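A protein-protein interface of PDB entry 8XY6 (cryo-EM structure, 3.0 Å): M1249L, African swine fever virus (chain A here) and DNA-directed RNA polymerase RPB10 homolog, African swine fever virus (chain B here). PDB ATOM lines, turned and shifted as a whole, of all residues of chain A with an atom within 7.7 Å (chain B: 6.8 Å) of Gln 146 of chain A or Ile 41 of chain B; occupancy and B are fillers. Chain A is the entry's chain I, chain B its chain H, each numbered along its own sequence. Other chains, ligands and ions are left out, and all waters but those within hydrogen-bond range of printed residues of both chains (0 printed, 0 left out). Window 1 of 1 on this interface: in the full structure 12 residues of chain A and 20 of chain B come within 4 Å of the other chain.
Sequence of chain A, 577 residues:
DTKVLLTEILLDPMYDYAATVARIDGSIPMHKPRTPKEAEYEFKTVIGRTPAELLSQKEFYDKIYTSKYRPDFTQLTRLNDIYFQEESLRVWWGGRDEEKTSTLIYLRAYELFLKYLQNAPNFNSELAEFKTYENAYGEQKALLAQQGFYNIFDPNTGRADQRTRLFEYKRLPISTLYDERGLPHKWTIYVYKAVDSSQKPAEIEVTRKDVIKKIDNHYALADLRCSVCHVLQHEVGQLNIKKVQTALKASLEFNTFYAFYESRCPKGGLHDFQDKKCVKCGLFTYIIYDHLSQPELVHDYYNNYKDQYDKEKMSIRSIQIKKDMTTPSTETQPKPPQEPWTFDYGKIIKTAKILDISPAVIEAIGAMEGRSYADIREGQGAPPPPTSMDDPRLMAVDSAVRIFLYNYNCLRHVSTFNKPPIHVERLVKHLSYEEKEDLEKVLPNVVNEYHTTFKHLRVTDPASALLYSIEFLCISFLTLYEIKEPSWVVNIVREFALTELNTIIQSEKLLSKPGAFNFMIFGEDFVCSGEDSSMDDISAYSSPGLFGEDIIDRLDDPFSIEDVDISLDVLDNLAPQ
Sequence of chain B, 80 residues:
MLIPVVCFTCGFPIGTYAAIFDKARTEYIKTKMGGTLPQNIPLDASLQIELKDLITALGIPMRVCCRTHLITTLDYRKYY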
ATOM      1  N   LYS A 141       9.663  15.390 -13.680  1.00  0.00           N
ATOM      2  CA  LYS A 141       9.791  14.178 -14.479  1.00  0.00           C
ATOM      3  C   LYS A 141      10.734  14.360 -15.662  1.00  0.00           C
ATOM      4  O   LYS A 141      11.337  13.383 -16.115  1.00  0.00           O
ATOM      5  CB  LYS A 141       8.421  13.723 -14.983  1.00  0.00           C
ATOM      6  CG  LYS A 141       8.287  12.217 -15.114  1.00  0.00           C
ATOM      7  CD  LYS A 141       6.835  11.777 -15.057  1.00  0.00           C
ATOM      8  CE  LYS A 141       6.266  11.585 -16.453  1.00  0.00           C
ATOM      9  NZ  LYS A 141       5.417  10.367 -16.549  1.00  0.00           N
ATOM     10  N   ALA A 142      10.865  15.585 -16.171  1.00  0.00           N
ATOM     11  CA  ALA A 142      11.825  15.855 -17.232  1.00  0.00           C
ATOM     12  C   ALA A 142      13.250  15.810 -16.711  1.00  0.00           C
ATOM     13  O   ALA A 142      14.182  15.553 -17.481  1.00  0.00           O
ATOM     14  CB  ALA A 142      11.538  17.212 -17.873  1.00  0.00           C
ATOM     15  N   LEU A 143      13.443  16.075 -15.419  1.00  0.00           N
ATOM     16  CA  LEU A 143      14.766  15.874 -14.837  1.00  0.00           C
ATOM     17  C   LEU A 143      15.169  14.406 -14.892  1.00  0.00           C
ATOM     18  O   LEU A 143      16.327  14.085 -15.183  1.00  0.00           O
ATOM     19  CB  LEU A 143      14.801  16.403 -13.404  1.00  0.00           C
ATOM     20  CG  LEU A 143      16.179  16.756 -12.838  1.00  0.00           C
ATOM     21  CD1 LEU A 143      17.023  15.549 -12.495  1.00  0.00           C
ATOM     22  CD2 LEU A 143      16.892  17.571 -13.885  1.00  0.00           C
ATOM     23  N   LEU A 144      14.230  13.501 -14.625  1.00  0.00           N
ATOM     24  CA  LEU A 144      14.524  12.077 -14.708  1.00  0.00           C
ATOM     25  C   LEU A 144      14.828  11.622 -16.128  1.00  0.00           C
ATOM     26  O   LEU A 144      15.371  10.527 -16.304  1.00  0.00           O
ATOM     27  CB  LEU A 144      13.355  11.266 -14.153  1.00  0.00           C
ATOM     28  CG  LEU A 144      12.788  11.705 -12.804  1.00  0.00           C
ATOM     29  CD1 LEU A 144      11.792  10.679 -12.289  1.00  0.00           C
ATOM     30  CD2 LEU A 144      13.896  11.932 -11.792  1.00  0.00           C
ATOM     31  N   ALA A 145      14.491  12.424 -17.139  1.00  0.00           N
ATOM     32  CA  ALA A 145      14.734  12.063 -18.528  1.00  0.00           C
ATOM     33  C   ALA A 145      16.084  12.524 -19.051  1.00  0.00           C
ATOM     34  O   ALA A 145      16.485  12.098 -20.137  1.00  0.00           O
ATOM     35  CB  ALA A 145      13.632  12.636 -19.426  1.00  0.00           C
ATOM     36  N   GLN A 146      16.792  13.376 -18.316  1.00  0.00           N
ATOM     37  CA  GLN A 146      18.079  13.865 -18.784  1.00  0.00           C
ATOM     38  C   GLN A 146      19.119  12.753 -18.738  1.00  0.00           C
ATOM     39  O   GLN A 146      19.246  12.049 -17.734  1.00  0.00           O
ATOM     40  CB  GLN A 146      18.533  15.049 -17.939  1.00  0.00           C
ATOM     41  CG  GLN A 146      17.943  16.371 -18.380  1.00  0.00           C
ATOM     42  CD  GLN A 146      18.005  16.553 -19.880  1.00  0.00           C
ATOM     43  OE1 GLN A 146      19.070  16.441 -20.485  1.00  0.00           O
ATOM     44  NE2 GLN A 146      16.861  16.839 -20.490  1.00  0.00           N
ATOM     45  N   GLN A 147      19.866  12.600 -19.831  1.00  0.00           N
ATOM     46  CA  GLN A 147      20.939  11.621 -19.913  1.00  0.00           C
ATOM     47  C   GLN A 147      22.324  12.232 -19.810  1.00  0.00           C
ATOM     48  O   GLN A 147      23.313  11.513 -19.982  1.00  0.00           O
ATOM     49  CB  GLN A 147      20.849  10.834 -21.227  1.00  0.00           C
ATOM     50  CG  GLN A 147      19.770   9.781 -21.244  1.00  0.00           C
ATOM     51  CD  GLN A 147      18.930   9.855 -22.490  1.00  0.00           C
ATOM     52  OE1 GLN A 147      19.441  10.111 -23.577  1.00  0.00           O
ATOM     53  NE2 GLN A 147      17.632   9.634 -22.343  1.00  0.00           N
ATOM     54  N   GLY A 148      22.428  13.525 -19.543  1.00  0.00           N
ATOM     55  CA  GLY A 148      23.705  14.200 -19.471  1.00  0.00           C
ATOM     56  C   GLY A 148      24.039  14.920 -20.764  1.00  0.00           C
ATOM     57  O   GLY A 148      23.407  14.735 -21.801  1.00  0.00           O
ATOM     58  N   PHE A 149      25.060  15.764 -20.667  1.00  0.00           N
ATOM     59  CA  PHE A 149      25.508  16.557 -21.805  1.00  0.00           C
ATOM     60  C   PHE A 149      26.874  17.126 -21.473  1.00  0.00           C
ATOM     61  O   PHE A 149      27.015  17.845 -20.482  1.00  0.00           O
ATOM     62  CB  PHE A 149      24.513  17.671 -22.107  1.00  0.00           C
ATOM     63  CG  PHE A 149      24.956  18.597 -23.188  1.00  0.00           C
ATOM     64  CD1 PHE A 149      24.903  18.206 -24.508  1.00  0.00           C
ATOM     65  CD2 PHE A 149      25.424  19.860 -22.886  1.00  0.00           C
ATOM     66  CE1 PHE A 149      25.310  19.053 -25.506  1.00  0.00           C
ATOM     67  CE2 PHE A 149      25.834  20.716 -23.883  1.00  0.00           C
ATOM     68  CZ  PHE A 149      25.776  20.312 -25.197  1.00  0.00           C
ATOM     69  N   TYR A 150      27.875  16.819 -22.290  1.00  0.00           N
ATOM     70  CA  TYR A 150      29.246  17.214 -22.012  1.00  0.00           C
ATOM     71  C   TYR A 150      29.708  18.185 -23.083  1.00  0.00           C
ATOM     72  O   TYR A 150      29.434  17.986 -24.269  1.00  0.00           O
ATOM     73  CB  TYR A 150      30.165  15.994 -21.964  1.00  0.00           C
ATOM     74  CG  TYR A 150      31.644  16.287 -22.064  1.00  0.00           C
ATOM     75  CD1 TYR A 150      32.375  16.649 -20.944  1.00  0.00           C
ATOM     76  CD2 TYR A 150      32.312  16.200 -23.276  1.00  0.00           C
ATOM     77  CE1 TYR A 150      33.726  16.918 -21.026  1.00  0.00           C
ATOM     78  CE2 TYR A 150      33.663  16.469 -23.366  1.00  0.00           C
ATOM     79  CZ  TYR A 150      34.364  16.827 -22.239  1.00  0.00           C
ATOM     80  OH  TYR A 150      35.708  17.092 -22.326  1.00  0.00           O
ATOM     81  N   ASN A 151      30.404  19.231 -22.662  1.00  0.00           N
ATOM     82  CA  ASN A 151      30.951  20.231 -23.565  1.00  0.00           C
ATOM     83  C   ASN A 151      32.464  20.083 -23.580  1.00  0.00           C
ATOM     84  O   ASN A 151      33.100  20.087 -22.523  1.00  0.00           O
ATOM     85  CB  ASN A 151      30.553  21.637 -23.125  1.00  0.00           C
ATOM     86  CG  ASN A 151      29.277  22.101 -23.775  1.00  0.00           C
ATOM     87  OD1 ASN A 151      28.382  22.610 -23.107  1.00  0.00           O
ATOM     88  ND2 ASN A 151      29.180  21.928 -25.085  1.00  0.00           N
ATOM     89  N   ASP B  22      20.148   4.246 -14.030  1.00  0.00           N
ATOM     90  CA  ASP B  22      19.228   5.372 -14.210  1.00  0.00           C
ATOM     91  C   ASP B  22      19.189   6.246 -12.964  1.00  0.00           C
ATOM     92  O   ASP B  22      19.349   7.469 -13.041  1.00  0.00           O
ATOM     93  CB  ASP B  22      17.805   4.930 -14.568  1.00  0.00           C
ATOM     94  CG  ASP B  22      17.755   3.788 -15.544  1.00  0.00           C
ATOM     95  OD1 ASP B  22      18.242   2.703 -15.215  1.00  0.00           O
ATOM     96  OD2 ASP B  22      17.161   3.957 -16.629  1.00  0.00           O
ATOM     97  N   ARG B  25      22.594   7.974 -12.314  1.00  0.00           N
ATOM     98  CA  ARG B  25      22.791   9.066 -13.252  1.00  0.00           C
ATOM     99  C   ARG B  25      21.922  10.258 -12.891  1.00  0.00           C
ATOM    100  O   ARG B  25      22.369  11.405 -12.970  1.00  0.00           O
ATOM    101  CB  ARG B  25      22.495   8.589 -14.672  1.00  0.00           C
ATOM    102  CG  ARG B  25      22.574   9.678 -15.712  1.00  0.00           C
ATOM    103  CD  ARG B  25      22.371   9.138 -17.107  1.00  0.00           C
ATOM    104  NE  ARG B  25      21.099   8.442 -17.238  1.00  0.00           N
ATOM    105  CZ  ARG B  25      20.751   7.720 -18.293  1.00  0.00           C
ATOM    106  NH1 ARG B  25      21.554   7.589 -19.334  1.00  0.00           N
ATOM    107  NH2 ARG B  25      19.568   7.116 -18.302  1.00  0.00           N
ATOM    108  N   THR B  26      20.674  10.010 -12.490  1.00  0.00           N
ATOM    109  CA  THR B  26      19.815  11.105 -12.052  1.00  0.00           C
ATOM    110  C   THR B  26      20.437  11.842 -10.875  1.00  0.00           C
ATOM    111  O   THR B  26      20.502  13.079 -10.859  1.00  0.00           O
ATOM    112  CB  THR B  26      18.438  10.563 -11.676  1.00  0.00           C
ATOM    113  OG1 THR B  26      17.891   9.837 -12.782  1.00  0.00           O
ATOM    114  CG2 THR B  26      17.508  11.693 -11.318  1.00  0.00           C
ATOM    115  N   ILE B  29      23.523  13.885 -12.097  1.00  0.00           N
ATOM    116  CA  ILE B  29      23.070  15.079 -12.805  1.00  0.00           C
ATOM    117  C   ILE B  29      22.577  16.130 -11.823  1.00  0.00           C
ATOM    118  O   ILE B  29      22.846  17.326 -11.987  1.00  0.00           O
ATOM    119  CB  ILE B  29      21.988  14.712 -13.842  1.00  0.00           C
ATOM    120  CG1 ILE B  29      22.614  14.385 -15.198  1.00  0.00           C
ATOM    121  CG2 ILE B  29      20.971  15.826 -13.984  1.00  0.00           C
ATOM    122  CD1 ILE B  29      23.308  13.078 -15.290  1.00  0.00           C
ATOM    123  N   LYS B  30      21.860  15.702 -10.780  1.00  0.00           N
ATOM    124  CA  LYS B  30      21.383  16.649  -9.778  1.00  0.00           C
ATOM    125  C   LYS B  30      22.525  17.481  -9.210  1.00  0.00           C
ATOM    126  O   LYS B  30      22.392  18.696  -9.038  1.00  0.00           O
ATOM    127  CB  LYS B  30      20.666  15.905  -8.656  1.00  0.00           C
ATOM    128  CG  LYS B  30      19.159  15.959  -8.736  1.00  0.00           C
ATOM    129  CD  LYS B  30      18.544  15.147  -7.619  1.00  0.00           C
ATOM    130  CE  LYS B  30      17.093  14.842  -7.902  1.00  0.00           C
ATOM    131  NZ  LYS B  30      16.949  13.945  -9.071  1.00  0.00           N
ATOM    132  N   MET B  33      24.341  19.748 -12.159  1.00  0.00           N
ATOM    133  CA  MET B  33      23.580  20.836 -12.745  1.00  0.00           C
ATOM    134  C   MET B  33      23.695  22.081 -11.875  1.00  0.00           C
ATOM    135  O   MET B  33      24.266  22.057 -10.781  1.00  0.00           O
ATOM    136  CB  MET B  33      22.110  20.458 -12.894  1.00  0.00           C
ATOM    137  CG  MET B  33      21.357  20.536 -11.587  1.00  0.00           C
ATOM    138  SD  MET B  33      19.574  20.509 -11.784  1.00  0.00           S
ATOM    139  CE  MET B  33      19.304  18.749 -11.801  1.00  0.00           C
ATOM    140  N   GLY B  34      23.141  23.179 -12.372  1.00  0.00           N
ATOM    141  CA  GLY B  34      23.131  24.407 -11.605  1.00  0.00           C
ATOM    142  C   GLY B  34      21.809  25.130 -11.701  1.00  0.00           C
ATOM    143  O   GLY B  34      20.747  24.514 -11.575  1.00  0.00           O
ATOM    144  N   THR B  36      19.753  25.741 -13.894  1.00  0.00           N
ATOM    145  CA  THR B  36      19.361  25.357 -15.244  1.00  0.00           C
ATOM    146  C   THR B  36      18.188  24.397 -15.155  1.00  0.00           C
ATOM    147  O   THR B  36      18.251  23.405 -14.426  1.00  0.00           O
ATOM    148  CB  THR B  36      20.528  24.709 -15.993  1.00  0.00           C
ATOM    149  OG1 THR B  36      21.465  25.719 -16.382  1.00  0.00           O
ATOM    150  CG2 THR B  36      20.030  23.988 -17.230  1.00  0.00           C
ATOM    151  N   LEU B  37      17.128  24.693 -15.897  1.00  0.00           N
ATOM    152  CA  LEU B  37      15.951  23.846 -15.874  1.00  0.00           C
ATOM    153  C   LEU B  37      16.268  22.493 -16.510  1.00  0.00           C
ATOM    154  O   LEU B  37      17.192  22.380 -17.316  1.00  0.00           O
ATOM    155  CB  LEU B  37      14.802  24.523 -16.614  1.00  0.00           C
ATOM    156  CG  LEU B  37      14.188  25.757 -15.953  1.00  0.00           C
ATOM    157  CD1 LEU B  37      12.726  25.867 -16.327  1.00  0.00           C
ATOM    158  CD2 LEU B  37      14.350  25.713 -14.447  1.00  0.00           C
ATOM    159  N   PRO B  38      15.527  21.443 -16.141  1.00  0.00           N
ATOM    160  CA  PRO B  38      15.811  20.117 -16.716  1.00  0.00           C
ATOM    161  C   PRO B  38      15.724  20.075 -18.230  1.00  0.00           C
ATOM    162  O   PRO B  38      16.542  19.408 -18.875  1.00  0.00           O
ATOM    163  CB  PRO B  38      14.747  19.225 -16.067  1.00  0.00           C
ATOM    164  CG  PRO B  38      14.313  19.957 -14.854  1.00  0.00           C
ATOM    165  CD  PRO B  38      14.418  21.401 -15.180  1.00  0.00           C
ATOM    166  N   GLN B  39      14.755  20.770 -18.823  1.00  0.00           N
ATOM    167  CA  GLN B  39      14.634  20.774 -20.272  1.00  0.00           C
ATOM    168  C   GLN B  39      15.715  21.603 -20.945  1.00  0.00           C
ATOM    169  O   GLN B  39      15.833  21.557 -22.173  1.00  0.00           O
ATOM    170  CB  GLN B  39      13.253  21.281 -20.690  1.00  0.00           C
ATOM    171  CG  GLN B  39      12.162  21.040 -19.663  1.00  0.00           C
ATOM    172  CD  GLN B  39      11.819  22.281 -18.873  1.00  0.00           C
ATOM    173  OE1 GLN B  39      12.679  23.117 -18.606  1.00  0.00           O
ATOM    174  NE2 GLN B  39      10.554  22.409 -18.492  1.00  0.00           N
ATOM    175  N   ASN B  40      16.491  22.360 -20.180  1.00  0.00           N
ATOM    176  CA  ASN B  40      17.592  23.142 -20.713  1.00  0.00           C
ATOM    177  C   ASN B  40      18.949  22.532 -20.398  1.00  0.00           C
ATOM    178  O   ASN B  40      19.973  23.110 -20.766  1.00  0.00           O
ATOM    179  CB  ASN B  40      17.524  24.570 -20.173  1.00  0.00           C
ATOM    180  CG  ASN B  40      16.185  25.223 -20.435  1.00  0.00           C
ATOM    181  OD1 ASN B  40      15.343  24.671 -21.140  1.00  0.00           O
ATOM    182  ND2 ASN B  40      15.975  26.395 -19.857  1.00  0.00           N
ATOM    183  N   ILE B  41      18.978  21.382 -19.719  1.00  0.00           N
ATOM    184  CA  ILE B  41      20.254  20.713 -19.451  1.00  0.00           C
ATOM    185  C   ILE B  41      20.994  20.375 -20.737  1.00  0.00           C
ATOM    186  O   ILE B  41      22.199  20.653 -20.817  1.00  0.00           O
ATOM    187  CB  ILE B  41      20.031  19.495 -18.544  1.00  0.00           C
ATOM    188  CG1 ILE B  41      20.075  19.910 -17.074  1.00  0.00           C
ATOM    189  CG2 ILE B  41      21.067  18.420 -18.819  1.00  0.00           C
ATOM    190  CD1 ILE B  41      20.018  18.746 -16.124  1.00  0.00           C
ATOM    191  N   PRO B  42      20.361  19.810 -21.788  1.00  0.00           N
ATOM    192  CA  PRO B  42      21.114  19.538 -23.021  1.00  0.00           C
ATOM    193  C   PRO B  42      21.393  20.797 -23.823  1.00  0.00           C
ATOM    194  O   PRO B  42      21.713  20.726 -25.012  1.00  0.00           O
ATOM    195  CB  PRO B  42      20.201  18.578 -23.791  1.00  0.00           C
ATOM    196  CG  PRO B  42      18.859  18.827 -23.271  1.00  0.00           C
ATOM    197  CD  PRO B  42      19.009  19.228 -21.845  1.00  0.00           C
ATOM    198  N   LEU B  43      21.249  21.956 -23.187  1.00  0.00           N
ATOM    199  CA  LEU B  43      21.530  23.229 -23.822  1.00  0.00           C
ATOM    200  C   LEU B  43      22.611  24.037 -23.122  1.00  0.00           C
ATOM    201  O   LEU B  43      23.043  25.059 -23.665  1.00  0.00           O
ATOM    202  CB  LEU B  43      20.256  24.075 -23.897  1.00  0.00           C
ATOM    203  CG  LEU B  43      19.505  24.048 -25.215  1.00  0.00           C
ATOM    204  CD1 LEU B  43      18.066  24.386 -24.950  1.00  0.00           C
ATOM    205  CD2 LEU B  43      20.129  25.053 -26.155  1.00  0.00           C
ATOM    206  N   ASP B  44      23.053  23.619 -21.942  1.00  0.00           N
ATOM    207  CA  ASP B  44      24.004  24.400 -21.162  1.00  0.00           C
ATOM    208  C   ASP B  44      25.383  24.340 -21.801  1.00  0.00           C
ATOM    209  O   ASP B  44      25.893  23.252 -22.088  1.00  0.00           O
ATOM    210  CB  ASP B  44      24.057  23.881 -19.732  1.00  0.00           C
ATOM    211  CG  ASP B  44      23.917  24.978 -18.705  1.00  0.00           C
ATOM    212  OD1 ASP B  44      24.572  26.029 -18.861  1.00  0.00           O
ATOM    213  OD2 ASP B  44      23.168  24.780 -17.729  1.00  0.00           O
ATOM    214  N   ALA B  45      25.990  25.506 -22.014  1.00  0.00           N
ATOM    215  CA  ALA B  45      27.325  25.599 -22.589  1.00  0.00           C
ATOM    216  C   ALA B  45      28.431  25.534 -21.547  1.00  0.00           C
ATOM    217  O   ALA B  45      29.609  25.541 -21.918  1.00  0.00           O
ATOM    218  CB  ALA B  45      27.461  26.893 -23.390  1.00  0.00           C
ATOM    219  N   LEU B  47      28.308  23.150 -18.927  1.00  0.00           N
ATOM    220  CA  LEU B  47      27.886  21.943 -18.230  1.00  0.00           C
ATOM    221  C   LEU B  47      28.598  20.752 -18.849  1.00  0.00           C
ATOM    222  O   LEU B  47      28.541  20.561 -20.068  1.00  0.00           O
ATOM    223  CB  LEU B  47      26.364  21.794 -18.317  1.00  0.00           C
ATOM    224  CG  LEU B  47      25.543  20.796 -17.506  1.00  0.00           C
ATOM    225  CD1 LEU B  47      24.065  21.093 -17.657  1.00  0.00           C
ATOM    226  CD2 LEU B  47      25.803  19.408 -18.004  1.00  0.00           C
ATOM    227  N   ILE B  49      29.082  16.544 -17.973  1.00  0.00           N
ATOM    228  CA  ILE B  49      28.711  15.405 -17.147  1.00  0.00           C
ATOM    229  C   ILE B  49      29.331  14.163 -17.767  1.00  0.00           C
ATOM    230  O   ILE B  49      28.908  13.707 -18.834  1.00  0.00           O
ATOM    231  CB  ILE B  49      27.194  15.269 -17.010  1.00  0.00           C
ATOM    232  CG1 ILE B  49      26.635  16.454 -16.228  1.00  0.00           C
ATOM    233  CG2 ILE B  49      26.827  13.944 -16.378  1.00  0.00           C
ATOM    234  CD1 ILE B  49      25.143  16.518 -16.222  1.00  0.00           C
ATOM    235  N   LYS B  78      10.097   7.837 -19.113  1.00  0.00           N
ATOM    236  CA  LYS B  78      10.524   9.215 -18.913  1.00  0.00           C
ATOM    237  C   LYS B  78       9.779  10.175 -19.829  1.00  0.00           C
ATOM    238  O   LYS B  78       9.562  11.336 -19.468  1.00  0.00           O
ATOM    239  CB  LYS B  78      12.030   9.329 -19.135  1.00  0.00           C
ATOM    240  CG  LYS B  78      12.860   9.204 -17.869  1.00  0.00           C
ATOM    241  CD  LYS B  78      12.616   7.901 -17.136  1.00  0.00           C
ATOM    242  CE  LYS B  78      13.588   7.738 -15.983  1.00  0.00           C
ATOM    243  NZ  LYS B  78      14.933   7.319 -16.449  1.00  0.00           N
ATOM    244  N   TYR B  79       9.374   9.715 -21.009  1.00  0.00           N
ATOM    245  CA  TYR B  79       8.720  10.594 -21.969  1.00  0.00           C
ATOM    246  C   TYR B  79       7.211  10.423 -21.997  1.00  0.00           C
ATOM    247  O   TYR B  79       6.490  11.413 -22.149  1.00  0.00           O
ATOM    248  CB  TYR B  79       9.296  10.366 -23.368  1.00  0.00           C
ATOM    249  CG  TYR B  79      10.769  10.672 -23.451  1.00  0.00           C
ATOM    250  CD1 TYR B  79      11.714   9.705 -23.155  1.00  0.00           C
ATOM    251  CD2 TYR B  79      11.215  11.935 -23.798  1.00  0.00           C
ATOM    252  CE1 TYR B  79      13.055   9.979 -23.215  1.00  0.00           C
ATOM    253  CE2 TYR B  79      12.557  12.220 -23.863  1.00  0.00           C
ATOM    254  CZ  TYR B  79      13.473  11.237 -23.571  1.00  0.00           C
ATOM    255  OH  TYR B  79      14.817  11.514 -23.633  1.00  0.00           O
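Of the 11 printed residues of chain A, 9 touch a printed residue of chain B. Hydrophobic or aromatic side chains of chain A within 4 Å of the printed part of chain B: Leu 143, Leu 144, Ala 145 and Phe 149. Along chain A the printed residues that touch a printed residue of chain B span positions 142 to 151. Of the 21 printed residues of chain B, 13 touch a printed residue of chain A. Hydrophobic or aromatic side chains of chain B that line the printed part of chain A: Met 33, Pro 38, Ile 41, Pro 42, Leu 47 and Tyr 79. Among the printed residues, no Asp or Glu carboxylate lies within 4 Å of a Lys or Arg side-chain nitrogen of the other chain.
Of the printed residues of chain B, Gln 146 of chain A touches Pro 38 (3.1 Å), Ile 41 (3.3 Å) and Pro 42 (3.1 Å). Of the printed residues of chain A, Pro 38 of chain B touches Ala 142 (3.8 Å), Leu 143 (3.5 Å) and Gln 146 (3.1 Å). Printed residues of chain A within 4 Å of Ile 41 of chain B: Gln 146 and Phe 149. Of the printed residues of chain A, Ile 49 of chain B touches Phe 149 (3.5 Å). The nearest residue of chain B that does not touch Gln 146 of chain A is Arg 25 of chain B (4.1 Å). The nearest residue of chain A that does not touch Ile 41 of chain B is Leu 143 of chain A (4.02 Å).
Among the printed residues, pairs that only touch across the chains: Ala 142 of chain A with Pro 38 of chain B (3.8 Å), Leu 143 of chain A with Lys 30 of chain B (3.8 Å), Leu 143 of chain A with Met 33 of chain B (3.4 Å), Leu 143 of chain A with Pro 38 of chain B (3.5 Å), Leu 144 of chain A with Thr 26 of chain B (3.7 Å), Ala 145 of chain A with Lys 78 of chain B (3.5 Å), Ala 145 of chain A with Tyr 79 of chain B (3.9 Å), Gln 146 of chain A with Ile 41 of chain B (3.3 Å), Gln 146 of chain A with Pro 42 of chain B (3.1 Å), Gln 147 of chain A with Arg 25 of chain B (3.4 Å), Gln 147 of chain A with Tyr 79 of chain B (3.6 Å), Phe 149 of chain A with Ile 41 of chain B (3.9 Å), Phe 149 of chain A with Pro 42 of chain B (3.96 Å), Phe 149 of chain A with Asp 44 of chain B (3.1 Å), Phe 149 of chain A with Ile 49 of chain B (3.5 Å) and Tyr 150 of chain A with Leu 47 of chain B (3.9 Å).
O of Asp 22 of chain B is in hydrogen-bond range of OG1 of Thr 26 of chain B, at 2.8 Å. The side-chain amide nitrogen (NE2) of Gln 147 of chain A sits close to the backbone carbonyl oxygen (O) of Ala 145 of chain A (3.5 Å).
The side-chain amide nitrogen of Gln 146 of chain A is in hydrogen-bond range of the backbone carbonyl oxygen of Pro 38 of chain B, 3.1 Å away. The backbone carbonyl oxygen (O) of Ala 45 of chain B sits close to the side-chain amide oxygen (OD1) of Asn 151 of chain A (3.4 Å). O of Asp 44 of chain B sits close to OD1 of Asn 151 of chain A. The backbone NH (N) of Asn 151 of chain A lies within hydrogen-bond range of the backbone carbonyl oxygen (O) of Leu 47 of chain B. The side-chain amino group (NZ) of Lys 78 of chain B sits at hydrogen-bond distance from the backbone carbonyl oxygen (O) of Leu 144 of chain A (3.2 Å). The backbone carbonyl oxygen (O) of Phe 149 of chain A sits close to the backbone carbonyl oxygen (O) of Leu 47 of chain B (3.1 Å).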
